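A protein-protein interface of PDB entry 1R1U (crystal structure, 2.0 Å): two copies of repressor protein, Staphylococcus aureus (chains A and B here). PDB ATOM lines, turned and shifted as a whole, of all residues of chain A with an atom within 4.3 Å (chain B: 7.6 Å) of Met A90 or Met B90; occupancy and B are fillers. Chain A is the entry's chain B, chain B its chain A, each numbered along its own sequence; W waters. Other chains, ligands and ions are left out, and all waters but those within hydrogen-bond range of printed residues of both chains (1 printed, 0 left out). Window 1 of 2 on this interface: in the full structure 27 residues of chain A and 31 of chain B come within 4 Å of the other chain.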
ATOM      1  N   PHE A  20      -6.789  20.514  -6.389  1.00  0.00           N
ATOM      2  CA  PHE A  20      -6.493  21.636  -5.554  1.00  0.00           C
ATOM      3  C   PHE A  20      -5.347  22.510  -6.124  1.00  0.00           C
ATOM      4  O   PHE A  20      -5.440  23.710  -6.004  1.00  0.00           O
ATOM      5  CB  PHE A  20      -6.259  21.205  -4.108  1.00  0.00           C
ATOM      6  CG  PHE A  20      -7.530  20.704  -3.367  1.00  0.00           C
ATOM      7  CD1 PHE A  20      -8.716  21.396  -3.405  1.00  0.00           C
ATOM      8  CD2 PHE A  20      -7.472  19.571  -2.559  1.00  0.00           C
ATOM      9  CE1 PHE A  20      -9.834  20.934  -2.679  1.00  0.00           C
ATOM     10  CE2 PHE A  20      -8.591  19.114  -1.867  1.00  0.00           C
ATOM     11  CZ  PHE A  20      -9.751  19.802  -1.942  1.00  0.00           C
ATOM     12  N   LEU A  23      -6.902  24.916  -8.430  1.00  0.00           N
ATOM     13  CA  LEU A  23      -7.724  25.907  -7.790  1.00  0.00           C
ATOM     14  C   LEU A  23      -6.878  26.951  -7.061  1.00  0.00           C
ATOM     15  O   LEU A  23      -7.360  27.978  -6.650  1.00  0.00           O
ATOM     16  CB  LEU A  23      -8.691  25.226  -6.845  1.00  0.00           C
ATOM     17  CG  LEU A  23      -9.815  24.456  -7.560  1.00  0.00           C
ATOM     18  CD1 LEU A  23     -10.542  23.406  -6.684  1.00  0.00           C
ATOM     19  CD2 LEU A  23     -10.792  25.365  -8.223  1.00  0.00           C
ATOM     20  N   HIS A  86     -20.552  18.087  -6.934  1.00  0.00           N
ATOM     21  CA  HIS A  86     -19.466  17.913  -5.973  1.00  0.00           C
ATOM     22  C   HIS A  86     -18.485  19.101  -6.076  1.00  0.00           C
ATOM     23  O   HIS A  86     -18.026  19.583  -5.099  1.00  0.00           O
ATOM     24  CB  HIS A  86     -18.755  16.542  -6.166  1.00  0.00           C
ATOM     25  CG  HIS A  86     -19.706  15.384  -6.286  1.00  0.00           C
ATOM     26  ND1 HIS A  86     -19.842  14.653  -7.452  1.00  0.00           N
ATOM     27  CD2 HIS A  86     -20.632  14.896  -5.419  1.00  0.00           C
ATOM     28  CE1 HIS A  86     -20.792  13.743  -7.286  1.00  0.00           C
ATOM     29  NE2 HIS A  86     -21.293  13.879  -6.068  1.00  0.00           N
ATOM     30  N   VAL A  87     -18.200  19.548  -7.297  1.00  0.00           N
ATOM     31  CA  VAL A  87     -17.296  20.648  -7.547  1.00  0.00           C
ATOM     32  C   VAL A  87     -18.007  21.880  -7.059  1.00  0.00           C
ATOM     33  O   VAL A  87     -17.430  22.678  -6.360  1.00  0.00           O
ATOM     34  CB  VAL A  87     -17.000  20.820  -9.040  1.00  0.00           C
ATOM     35  CG1 VAL A  87     -16.342  22.226  -9.310  1.00  0.00           C
ATOM     36  CG2 VAL A  87     -16.108  19.691  -9.553  1.00  0.00           C
ATOM     37  N   ALA A  88     -19.284  22.046  -7.414  1.00  0.00           N
ATOM     38  CA  ALA A  88     -20.037  23.194  -6.899  1.00  0.00           C
ATOM     39  C   ALA A  88     -20.076  23.236  -5.377  1.00  0.00           C
ATOM     40  O   ALA A  88     -19.861  24.295  -4.724  1.00  0.00           O
ATOM     41  CB  ALA A  88     -21.461  23.174  -7.458  1.00  0.00           C
ATOM     42  N   THR A  89     -20.288  22.071  -4.762  1.00  0.00           N
ATOM     43  CA  THR A  89     -20.429  22.044  -3.317  1.00  0.00           C
ATOM     44  C   THR A  89     -19.092  22.345  -2.656  1.00  0.00           C
ATOM     45  O   THR A  89     -19.020  23.053  -1.660  1.00  0.00           O
ATOM     46  CB  THR A  89     -21.011  20.672  -2.841  1.00  0.00           C
ATOM     47  OG1 THR A  89     -22.308  20.456  -3.401  1.00  0.00           O
ATOM     48  CG2 THR A  89     -21.311  20.701  -1.428  1.00  0.00           C
ATOM     49  N   MET A  90     -18.027  21.784  -3.199  1.00  0.00           N
ATOM     50  CA  MET A  90     -16.670  22.015  -2.641  1.00  0.00           C
ATOM     51  C   MET A  90     -16.419  23.512  -2.673  1.00  0.00           C
ATOM     52  O   MET A  90     -16.022  24.126  -1.665  1.00  0.00           O
ATOM     53  CB  MET A  90     -15.665  21.220  -3.495  1.00  0.00           C
ATOM     54  CG  MET A  90     -14.232  21.581  -3.314  1.00  0.00           C
ATOM     55  SD  MET A  90     -13.258  21.158  -4.740  1.00  0.00           S
ATOM     56  CE  MET A  90     -13.652  22.561  -5.668  1.00  0.00           C
ATOM     57  N   LEU A  91     -16.703  24.114  -3.826  1.00  0.00           N
ATOM     58  CA  LEU A  91     -16.415  25.530  -4.030  1.00  0.00           C
ATOM     59  C   LEU A  91     -17.208  26.407  -3.124  1.00  0.00           C
ATOM     60  O   LEU A  91     -16.666  27.353  -2.477  1.00  0.00           O
ATOM     61  CB  LEU A  91     -16.610  25.960  -5.485  1.00  0.00           C
ATOM     62  CG  LEU A  91     -16.002  27.349  -5.766  1.00  0.00           C
ATOM     63  CD1 LEU A  91     -14.474  27.265  -5.951  1.00  0.00           C
ATOM     64  CD2 LEU A  91     -16.600  27.890  -7.002  1.00  0.00           C
ATOM     65  N   LYS A  92     -18.521  26.120  -3.012  1.00  0.00           N
ATOM     66  CA  LYS A  92     -19.362  27.026  -2.233  1.00  0.00           C
ATOM     67  C   LYS A  92     -19.025  26.909  -0.764  1.00  0.00           C
ATOM     68  O   LYS A  92     -19.165  27.874   0.031  1.00  0.00           O
ATOM     69  CB  LYS A  92     -20.893  26.724  -2.468  1.00  0.00           C
ATOM     70  CG  LYS A  92     -21.341  27.162  -3.830  1.00  0.00           C
ATOM     71  CD  LYS A  92     -22.841  26.846  -4.034  1.00  0.00           C
ATOM     72  CE  LYS A  92     -23.197  26.643  -5.500  1.00  0.00           C
ATOM     73  NZ  LYS A  92     -24.002  25.397  -5.735  1.00  0.00           N
ATOM     74  N   GLN A  93     -18.647  25.714  -0.328  1.00  0.00           N
ATOM     75  CA  GLN A  93     -18.426  25.556   1.092  1.00  0.00           C
ATOM     76  C   GLN A  93     -17.100  26.291   1.454  1.00  0.00           C
ATOM     77  O   GLN A  93     -16.973  26.931   2.485  1.00  0.00           O
ATOM     78  CB  GLN A  93     -18.362  24.066   1.455  1.00  0.00           C
ATOM     79  CG  GLN A  93     -19.723  23.326   1.319  1.00  0.00           C
ATOM     80  CD  GLN A  93     -20.589  23.395   2.578  1.00  0.00           C
ATOM     81  OE1 GLN A  93     -20.071  23.370   3.674  1.00  0.00           O
ATOM     82  NE2 GLN A  93     -21.956  23.460   2.401  1.00  0.00           N
ATOM     83  N   ALA A  94     -16.107  26.172   0.575  1.00  0.00           N
ATOM     84  CA  ALA A  94     -14.792  26.870   0.756  1.00  0.00           C
ATOM     85  C   ALA A  94     -14.999  28.397   0.831  1.00  0.00           C
ATOM     86  O   ALA A  94     -14.406  29.070   1.660  1.00  0.00           O
ATOM     87  CB  ALA A  94     -13.878  26.539  -0.410  1.00  0.00           C
ATOM     88  N   VAL B  16      -9.769  32.483   0.015  1.00  0.00           N
ATOM     89  CA  VAL B  16      -9.991  31.172  -0.614  1.00  0.00           C
ATOM     90  C   VAL B  16      -8.898  30.746  -1.563  1.00  0.00           C
ATOM     91  O   VAL B  16      -8.642  29.552  -1.714  1.00  0.00           O
ATOM     92  CB  VAL B  16     -11.411  30.901  -1.239  1.00  0.00           C
ATOM     93  CG1 VAL B  16     -12.402  31.982  -0.964  1.00  0.00           C
ATOM     94  CG2 VAL B  16     -11.357  30.536  -2.679  1.00  0.00           C
ATOM     95  N   ILE B  19      -6.486  29.262   0.752  1.00  0.00           N
ATOM     96  CA  ILE B  19      -6.991  27.950   1.167  1.00  0.00           C
ATOM     97  C   ILE B  19      -6.621  26.913   0.159  1.00  0.00           C
ATOM     98  O   ILE B  19      -6.122  25.855   0.499  1.00  0.00           O
ATOM     99  CB  ILE B  19      -8.528  27.998   1.431  1.00  0.00           C
ATOM    100  CG1 ILE B  19      -8.762  28.581   2.846  1.00  0.00           C
ATOM    101  CG2 ILE B  19      -9.162  26.633   1.262  1.00  0.00           C
ATOM    102  CD1 ILE B  19     -10.134  29.112   3.042  1.00  0.00           C
ATOM    103  N   PHE B  20      -6.846  27.220  -1.097  1.00  0.00           N
ATOM    104  CA  PHE B  20      -6.587  26.278  -2.135  1.00  0.00           C
ATOM    105  C   PHE B  20      -5.091  26.057  -2.428  1.00  0.00           C
ATOM    106  O   PHE B  20      -4.696  24.923  -2.725  1.00  0.00           O
ATOM    107  CB  PHE B  20      -7.394  26.621  -3.347  1.00  0.00           C
ATOM    108  CG  PHE B  20      -8.919  26.294  -3.205  1.00  0.00           C
ATOM    109  CD1 PHE B  20      -9.363  25.156  -2.587  1.00  0.00           C
ATOM    110  CD2 PHE B  20      -9.873  27.132  -3.761  1.00  0.00           C
ATOM    111  CE1 PHE B  20     -10.726  24.886  -2.490  1.00  0.00           C
ATOM    112  CE2 PHE B  20     -11.219  26.851  -3.673  1.00  0.00           C
ATOM    113  CZ  PHE B  20     -11.641  25.739  -3.014  1.00  0.00           C
ATOM    114  N   LEU B  23      -3.906  23.609   0.074  1.00  0.00           N
ATOM    115  CA  LEU B  23      -4.336  22.259  -0.203  1.00  0.00           C
ATOM    116  C   LEU B  23      -3.630  21.609  -1.386  1.00  0.00           C
ATOM    117  O   LEU B  23      -3.826  20.469  -1.705  1.00  0.00           O
ATOM    118  CB  LEU B  23      -5.828  22.259  -0.416  1.00  0.00           C
ATOM    119  CG  LEU B  23      -6.578  22.544   0.921  1.00  0.00           C
ATOM    120  CD1 LEU B  23      -8.060  22.914   0.700  1.00  0.00           C
ATOM    121  CD2 LEU B  23      -6.449  21.384   1.880  1.00  0.00           C
ATOM    122  N   MET B  32      -5.024  16.192   5.820  1.00  0.00           N
ATOM    123  CA  MET B  32      -6.461  16.553   5.852  1.00  0.00           C
ATOM    124  C   MET B  32      -7.433  15.389   5.811  1.00  0.00           C
ATOM    125  O   MET B  32      -8.506  15.432   6.483  1.00  0.00           O
ATOM    126  CB  MET B  32      -6.805  17.523   4.728  1.00  0.00           C
ATOM    127  CG  MET B  32      -6.106  18.868   4.844  1.00  0.00           C
ATOM    128  SD  MET B  32      -6.642  19.930   6.121  1.00  0.00           S
ATOM    129  CE  MET B  32      -8.295  20.413   5.383  1.00  0.00           C
ATOM    130  N   LEU B  68      -7.653  25.925   8.032  1.00  0.00           N
ATOM    131  CA  LEU B  68      -8.165  24.669   7.599  1.00  0.00           C
ATOM    132  C   LEU B  68      -8.116  23.599   8.714  1.00  0.00           C
ATOM    133  O   LEU B  68      -8.851  22.613   8.693  1.00  0.00           O
ATOM    134  CB  LEU B  68      -7.398  24.193   6.357  1.00  0.00           C
ATOM    135  CG  LEU B  68      -7.702  24.952   5.074  1.00  0.00           C
ATOM    136  CD1 LEU B  68      -6.719  24.565   3.993  1.00  0.00           C
ATOM    137  CD2 LEU B  68      -9.098  24.587   4.610  1.00  0.00           C
ATOM    138  N   LEU B  82      -9.934  19.078  11.557  1.00  0.00           N
ATOM    139  CA  LEU B  82     -10.450  19.980  10.543  1.00  0.00           C
ATOM    140  C   LEU B  82     -11.159  21.148  11.230  1.00  0.00           C
ATOM    141  O   LEU B  82     -11.758  20.970  12.268  1.00  0.00           O
ATOM    142  CB  LEU B  82     -11.394  19.237   9.667  1.00  0.00           C
ATOM    143  CG  LEU B  82     -10.952  18.535   8.397  1.00  0.00           C
ATOM    144  CD1 LEU B  82      -9.421  18.333   8.210  1.00  0.00           C
ATOM    145  CD2 LEU B  82     -11.727  17.335   8.206  1.00  0.00           C
ATOM    146  N   ASP B  84     -13.835  23.180  10.609  1.00  0.00           N
ATOM    147  CA  ASP B  84     -15.282  23.072  10.791  1.00  0.00           C
ATOM    148  C   ASP B  84     -15.885  22.214   9.740  1.00  0.00           C
ATOM    149  O   ASP B  84     -15.179  21.714   8.889  1.00  0.00           O
ATOM    150  CB  ASP B  84     -15.893  24.477  10.845  1.00  0.00           C
ATOM    151  CG  ASP B  84     -15.826  25.202   9.535  1.00  0.00           C
ATOM    152  OD1 ASP B  84     -16.112  26.438   9.576  1.00  0.00           O
ATOM    153  OD2 ASP B  84     -15.550  24.669   8.423  1.00  0.00           O
ATOM    154  N   ILE B  85     -17.211  22.119   9.719  1.00  0.00           N
ATOM    155  CA  ILE B  85     -17.919  21.304   8.713  1.00  0.00           C
ATOM    156  C   ILE B  85     -17.741  21.746   7.286  1.00  0.00           C
ATOM    157  O   ILE B  85     -17.923  20.990   6.391  1.00  0.00           O
ATOM    158  CB  ILE B  85     -19.477  21.282   9.026  1.00  0.00           C
ATOM    159  CG1 ILE B  85     -20.249  20.327   8.094  1.00  0.00           C
ATOM    160  CG2 ILE B  85     -20.044  22.679   8.985  1.00  0.00           C
ATOM    161  CD1 ILE B  85     -21.639  19.922   8.680  1.00  0.00           C
ATOM    162  N   HIS B  86     -17.563  23.018   7.060  1.00  0.00           N
ATOM    163  CA  HIS B  86     -17.420  23.487   5.709  1.00  0.00           C
ATOM    164  C   HIS B  86     -16.098  22.955   5.120  1.00  0.00           C
ATOM    165  O   HIS B  86     -16.067  22.542   3.990  1.00  0.00           O
ATOM    166  CB  HIS B  86     -17.497  25.023   5.646  1.00  0.00           C
ATOM    167  CG  HIS B  86     -18.581  25.616   6.491  1.00  0.00           C
ATOM    168  ND1 HIS B  86     -18.314  26.461   7.554  1.00  0.00           N
ATOM    169  CD2 HIS B  86     -19.924  25.514   6.416  1.00  0.00           C
ATOM    170  CE1 HIS B  86     -19.457  26.846   8.101  1.00  0.00           C
ATOM    171  NE2 HIS B  86     -20.448  26.270   7.439  1.00  0.00           N
ATOM    172  N   VAL B  87     -15.021  22.981   5.908  1.00  0.00           N
ATOM    173  CA  VAL B  87     -13.742  22.375   5.483  1.00  0.00           C
ATOM    174  C   VAL B  87     -13.916  20.872   5.253  1.00  0.00           C
ATOM    175  O   VAL B  87     -13.501  20.306   4.217  1.00  0.00           O
ATOM    176  CB  VAL B  87     -12.660  22.616   6.534  1.00  0.00           C
ATOM    177  CG1 VAL B  87     -11.390  21.709   6.240  1.00  0.00           C
ATOM    178  CG2 VAL B  87     -12.303  24.106   6.611  1.00  0.00           C
ATOM    179  N   ALA B  88     -14.551  20.185   6.200  1.00  0.00           N
ATOM    180  CA  ALA B  88     -14.831  18.768   6.011  1.00  0.00           C
ATOM    181  C   ALA B  88     -15.640  18.527   4.784  1.00  0.00           C
ATOM    182  O   ALA B  88     -15.386  17.566   4.036  1.00  0.00           O
ATOM    183  CB  ALA B  88     -15.567  18.197   7.224  1.00  0.00           C
ATOM    184  N   THR B  89     -16.630  19.380   4.524  1.00  0.00           N
ATOM    185  CA  THR B  89     -17.532  19.109   3.415  1.00  0.00           C
ATOM    186  C   THR B  89     -16.790  19.336   2.088  1.00  0.00           C
ATOM    187  O   THR B  89     -16.930  18.546   1.163  1.00  0.00           O
ATOM    188  CB  THR B  89     -18.841  19.970   3.490  1.00  0.00           C
ATOM    189  OG1 THR B  89     -19.596  19.704   4.693  1.00  0.00           O
ATOM    190  CG2 THR B  89     -19.742  19.584   2.461  1.00  0.00           C
ATOM    191  N   MET B  90     -16.014  20.426   2.017  1.00  0.00           N
ATOM    192  CA  MET B  90     -15.200  20.763   0.827  1.00  0.00           C
ATOM    193  C   MET B  90     -14.320  19.590   0.527  1.00  0.00           C
ATOM    194  O   MET B  90     -14.306  19.084  -0.567  1.00  0.00           O
ATOM    195  CB  MET B  90     -14.377  22.035   1.086  1.00  0.00           C
ATOM    196  CG  MET B  90     -13.194  22.261   0.166  1.00  0.00           C
ATOM    197  SD  MET B  90     -12.044  23.415   0.925  1.00  0.00           S
ATOM    198  CE  MET B  90     -11.167  22.303   1.999  1.00  0.00           C
ATOM    199  N   LEU B  91     -13.624  19.110   1.528  1.00  0.00           N
ATOM    200  CA  LEU B  91     -12.701  17.992   1.290  1.00  0.00           C
ATOM    201  C   LEU B  91     -13.357  16.730   0.853  1.00  0.00           C
ATOM    202  O   LEU B  91     -12.889  16.038  -0.112  1.00  0.00           O
ATOM    203  CB  LEU B  91     -11.853  17.711   2.517  1.00  0.00           C
ATOM    204  CG  LEU B  91     -10.652  16.760   2.331  1.00  0.00           C
ATOM    205  CD1 LEU B  91      -9.540  17.483   1.593  1.00  0.00           C
ATOM    206  CD2 LEU B  91     -10.137  16.366   3.711  1.00  0.00           C
ATOM    207  N   LYS B  92     -14.454  16.362   1.539  1.00  0.00           N
ATOM    208  CA  LYS B  92     -15.072  15.065   1.235  1.00  0.00           C
ATOM    209  C   LYS B  92     -15.673  15.098  -0.156  1.00  0.00           C
ATOM    210  O   LYS B  92     -15.730  14.081  -0.870  1.00  0.00           O
ATOM    211  CB  LYS B  92     -16.156  14.694   2.303  1.00  0.00           C
ATOM    212  CG  LYS B  92     -15.508  14.154   3.550  1.00  0.00           C
ATOM    213  CD  LYS B  92     -16.485  13.326   4.433  1.00  0.00           C
ATOM    214  CE  LYS B  92     -16.189  13.550   5.938  1.00  0.00           C
ATOM    215  NZ  LYS B  92     -16.900  14.732   6.556  1.00  0.00           N
ATOM    216  N   GLN B  93     -16.188  16.246  -0.567  1.00  0.00           N
ATOM    217  CA  GLN B  93     -16.835  16.296  -1.881  1.00  0.00           C
ATOM    218  C   GLN B  93     -15.766  16.253  -2.958  1.00  0.00           C
ATOM    219  O   GLN B  93     -15.950  15.587  -3.986  1.00  0.00           O
ATOM    220  CB  GLN B  93     -17.673  17.551  -2.054  1.00  0.00           C
ATOM    221  CG  GLN B  93     -18.862  17.665  -1.070  1.00  0.00           C
ATOM    222  CD  GLN B  93     -20.114  17.002  -1.611  1.00  0.00           C
ATOM    223  OE1 GLN B  93     -20.441  17.145  -2.820  1.00  0.00           O
ATOM    224  NE2 GLN B  93     -20.816  16.248  -0.733  1.00  0.00           N
ATOM    225  N   ALA B  94     -14.652  16.963  -2.728  1.00  0.00           N
ATOM    226  CA  ALA B  94     -13.481  16.910  -3.684  1.00  0.00           C
ATOM    227  C   ALA B  94     -12.949  15.457  -3.831  1.00  0.00           C
ATOM    228  O   ALA B  94     -12.731  14.981  -4.940  1.00  0.00           O
ATOM    229  CB  ALA B  94     -12.397  17.833  -3.199  1.00  0.00           C
ATOM    230  N   ILE B  95     -12.791  14.740  -2.735  1.00  0.00           N
ATOM    231  CA  ILE B  95     -12.326  13.334  -2.743  1.00  0.00           C
ATOM    232  C   ILE B  95     -13.269  12.479  -3.563  1.00  0.00           C
ATOM    233  O   ILE B  95     -12.845  11.698  -4.464  1.00  0.00           O
ATOM    234  CB  ILE B  95     -12.238  12.746  -1.323  1.00  0.00           C
ATOM    235  CG1 ILE B  95     -11.215  13.437  -0.421  1.00  0.00           C
ATOM    236  CG2 ILE B  95     -11.959  11.224  -1.361  1.00  0.00           C
ATOM    237  CD1 ILE B  95      -9.947  13.694  -0.998  1.00  0.00           C
ATOM    238  N   HIS B  96     -14.562  12.642  -3.296  1.00  0.00           N
ATOM    239  CA  HIS B  96     -15.572  11.869  -3.967  1.00  0.00           C
ATOM    240  C   HIS B  96     -15.526  12.117  -5.490  1.00  0.00           C
ATOM    241  O   HIS B  96     -15.570  11.166  -6.330  1.00  0.00           O
ATOM    242  CB  HIS B  96     -16.977  12.127  -3.334  1.00  0.00           C
ATOM    243  CG  HIS B  96     -18.067  11.399  -4.054  1.00  0.00           C
ATOM    244  ND1 HIS B  96     -18.054  10.033  -4.222  1.00  0.00           N
ATOM    245  CD2 HIS B  96     -19.132  11.846  -4.751  1.00  0.00           C
ATOM    246  CE1 HIS B  96     -19.077   9.667  -4.968  1.00  0.00           C
ATOM    247  NE2 HIS B  96     -19.758  10.744  -5.290  1.00  0.00           N
ATOM    248  N   HIS B  97     -15.396  13.386  -5.875  1.00  0.00           N
ATOM    249  CA  HIS B  97     -15.258  13.725  -7.291  1.00  0.00           C
ATOM    250  C   HIS B  97     -14.060  13.096  -7.945  1.00  0.00           C
ATOM    251  O   HIS B  97     -14.151  12.597  -9.060  1.00  0.00           O
ATOM    252  CB  HIS B  97     -15.163  15.229  -7.497  1.00  0.00           C
ATOM    253  CG  HIS B  97     -15.131  15.633  -8.922  1.00  0.00           C
ATOM    254  ND1 HIS B  97     -16.269  15.942  -9.615  1.00  0.00           N
ATOM    255  CD2 HIS B  97     -14.113  15.733  -9.814  1.00  0.00           C
ATOM    256  CE1 HIS B  97     -15.951  16.333 -10.832  1.00  0.00           C
ATOM    257  NE2 HIS B  97     -14.652  16.186 -10.991  1.00  0.00           N
HETATM  258  O   HOH W   1      -3.156  24.789  -4.954  1.00  0.00           O
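OD2 of Asp B84 lies within hydrogen-bond range of N of His B86 (2.9 Å). O of Ile B85 sits at hydrogen-bond distance from OG1 of Thr B89 (2.7 Å).
Water W1 bridges O of Phe B20 (2.7 Å) and O of Phe A20 (2.7 Å).
Of chain B, only Met B90 and Ala B94 come within 4 Å of Met A90. Of the printed residues of chain B, Thr A89 touches Gln B93 (3.6 Å). Of the printed residues of chain A, Phe B20 touches Phe A20 (3.6 Å), Leu A23 (3.6 Å), Leu A91 (3.99 Å) and Ala A94 (3.5 Å). Of the printed residues of chain B, Phe A20 touches Phe B20 (3.6 Å), Leu B23 (3.5 Å), Leu B91 (3.9 Å) and Ala B94 (3.5 Å). Asp B84 touches none of the printed residues of chain A. The nearest residue of chain B that does not touch Met A90 is Gln B93 (4.4 Å). The nearest printed residue of chain A that does not touch Met B90 is Gln A93 (4.4 Å).
Hydrophobic or aromatic side chains of chain B within 4 Å of the printed part of chain A: Phe B20, Leu B23, His B86, Met B90, Leu B91, Ala B94, His B96 and His B97. Of the 11 printed residues of chain A, 9 touch a printed residue of chain B.
O of Phe B20 touches O of Phe A20 (3.6 Å). Leu B91 touches Phe A20 (CD1 to CE2, 3.9 Å). Phe A20 touches Ala B94 (CZ to CB, 3.5 Å). O of Leu A23 touches CB of Phe B20, at 3.6 Å. CD2 of His B96 touches NE2 of His A86, 3.2 Å away. Val A87 touches His B97. Thr A89 touches Gln B93 (CB to OE1, 3.6 Å). His B86 touches Gln A93 (CA to OE1, 3.3 Å). Gln A93 touches Thr B89. Phe B20 touches Ala A94 (CZ to CB, 3.5 Å).
Phe A20 touches its own counterpart, Phe B20. Phe A20 touches Leu B23, and with the chains exchanged Leu A23 touches Phe B20. His A86 touches Gln B93, and with the chains exchanged Gln A93 touches His B86. Met A90 touches Ala B94, and with the chains exchanged Ala A94 touches Met B90. Positions printed for both chains: 20, 23, 86, 87, 88, 89, 90, 91, 92, 93 and 94.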
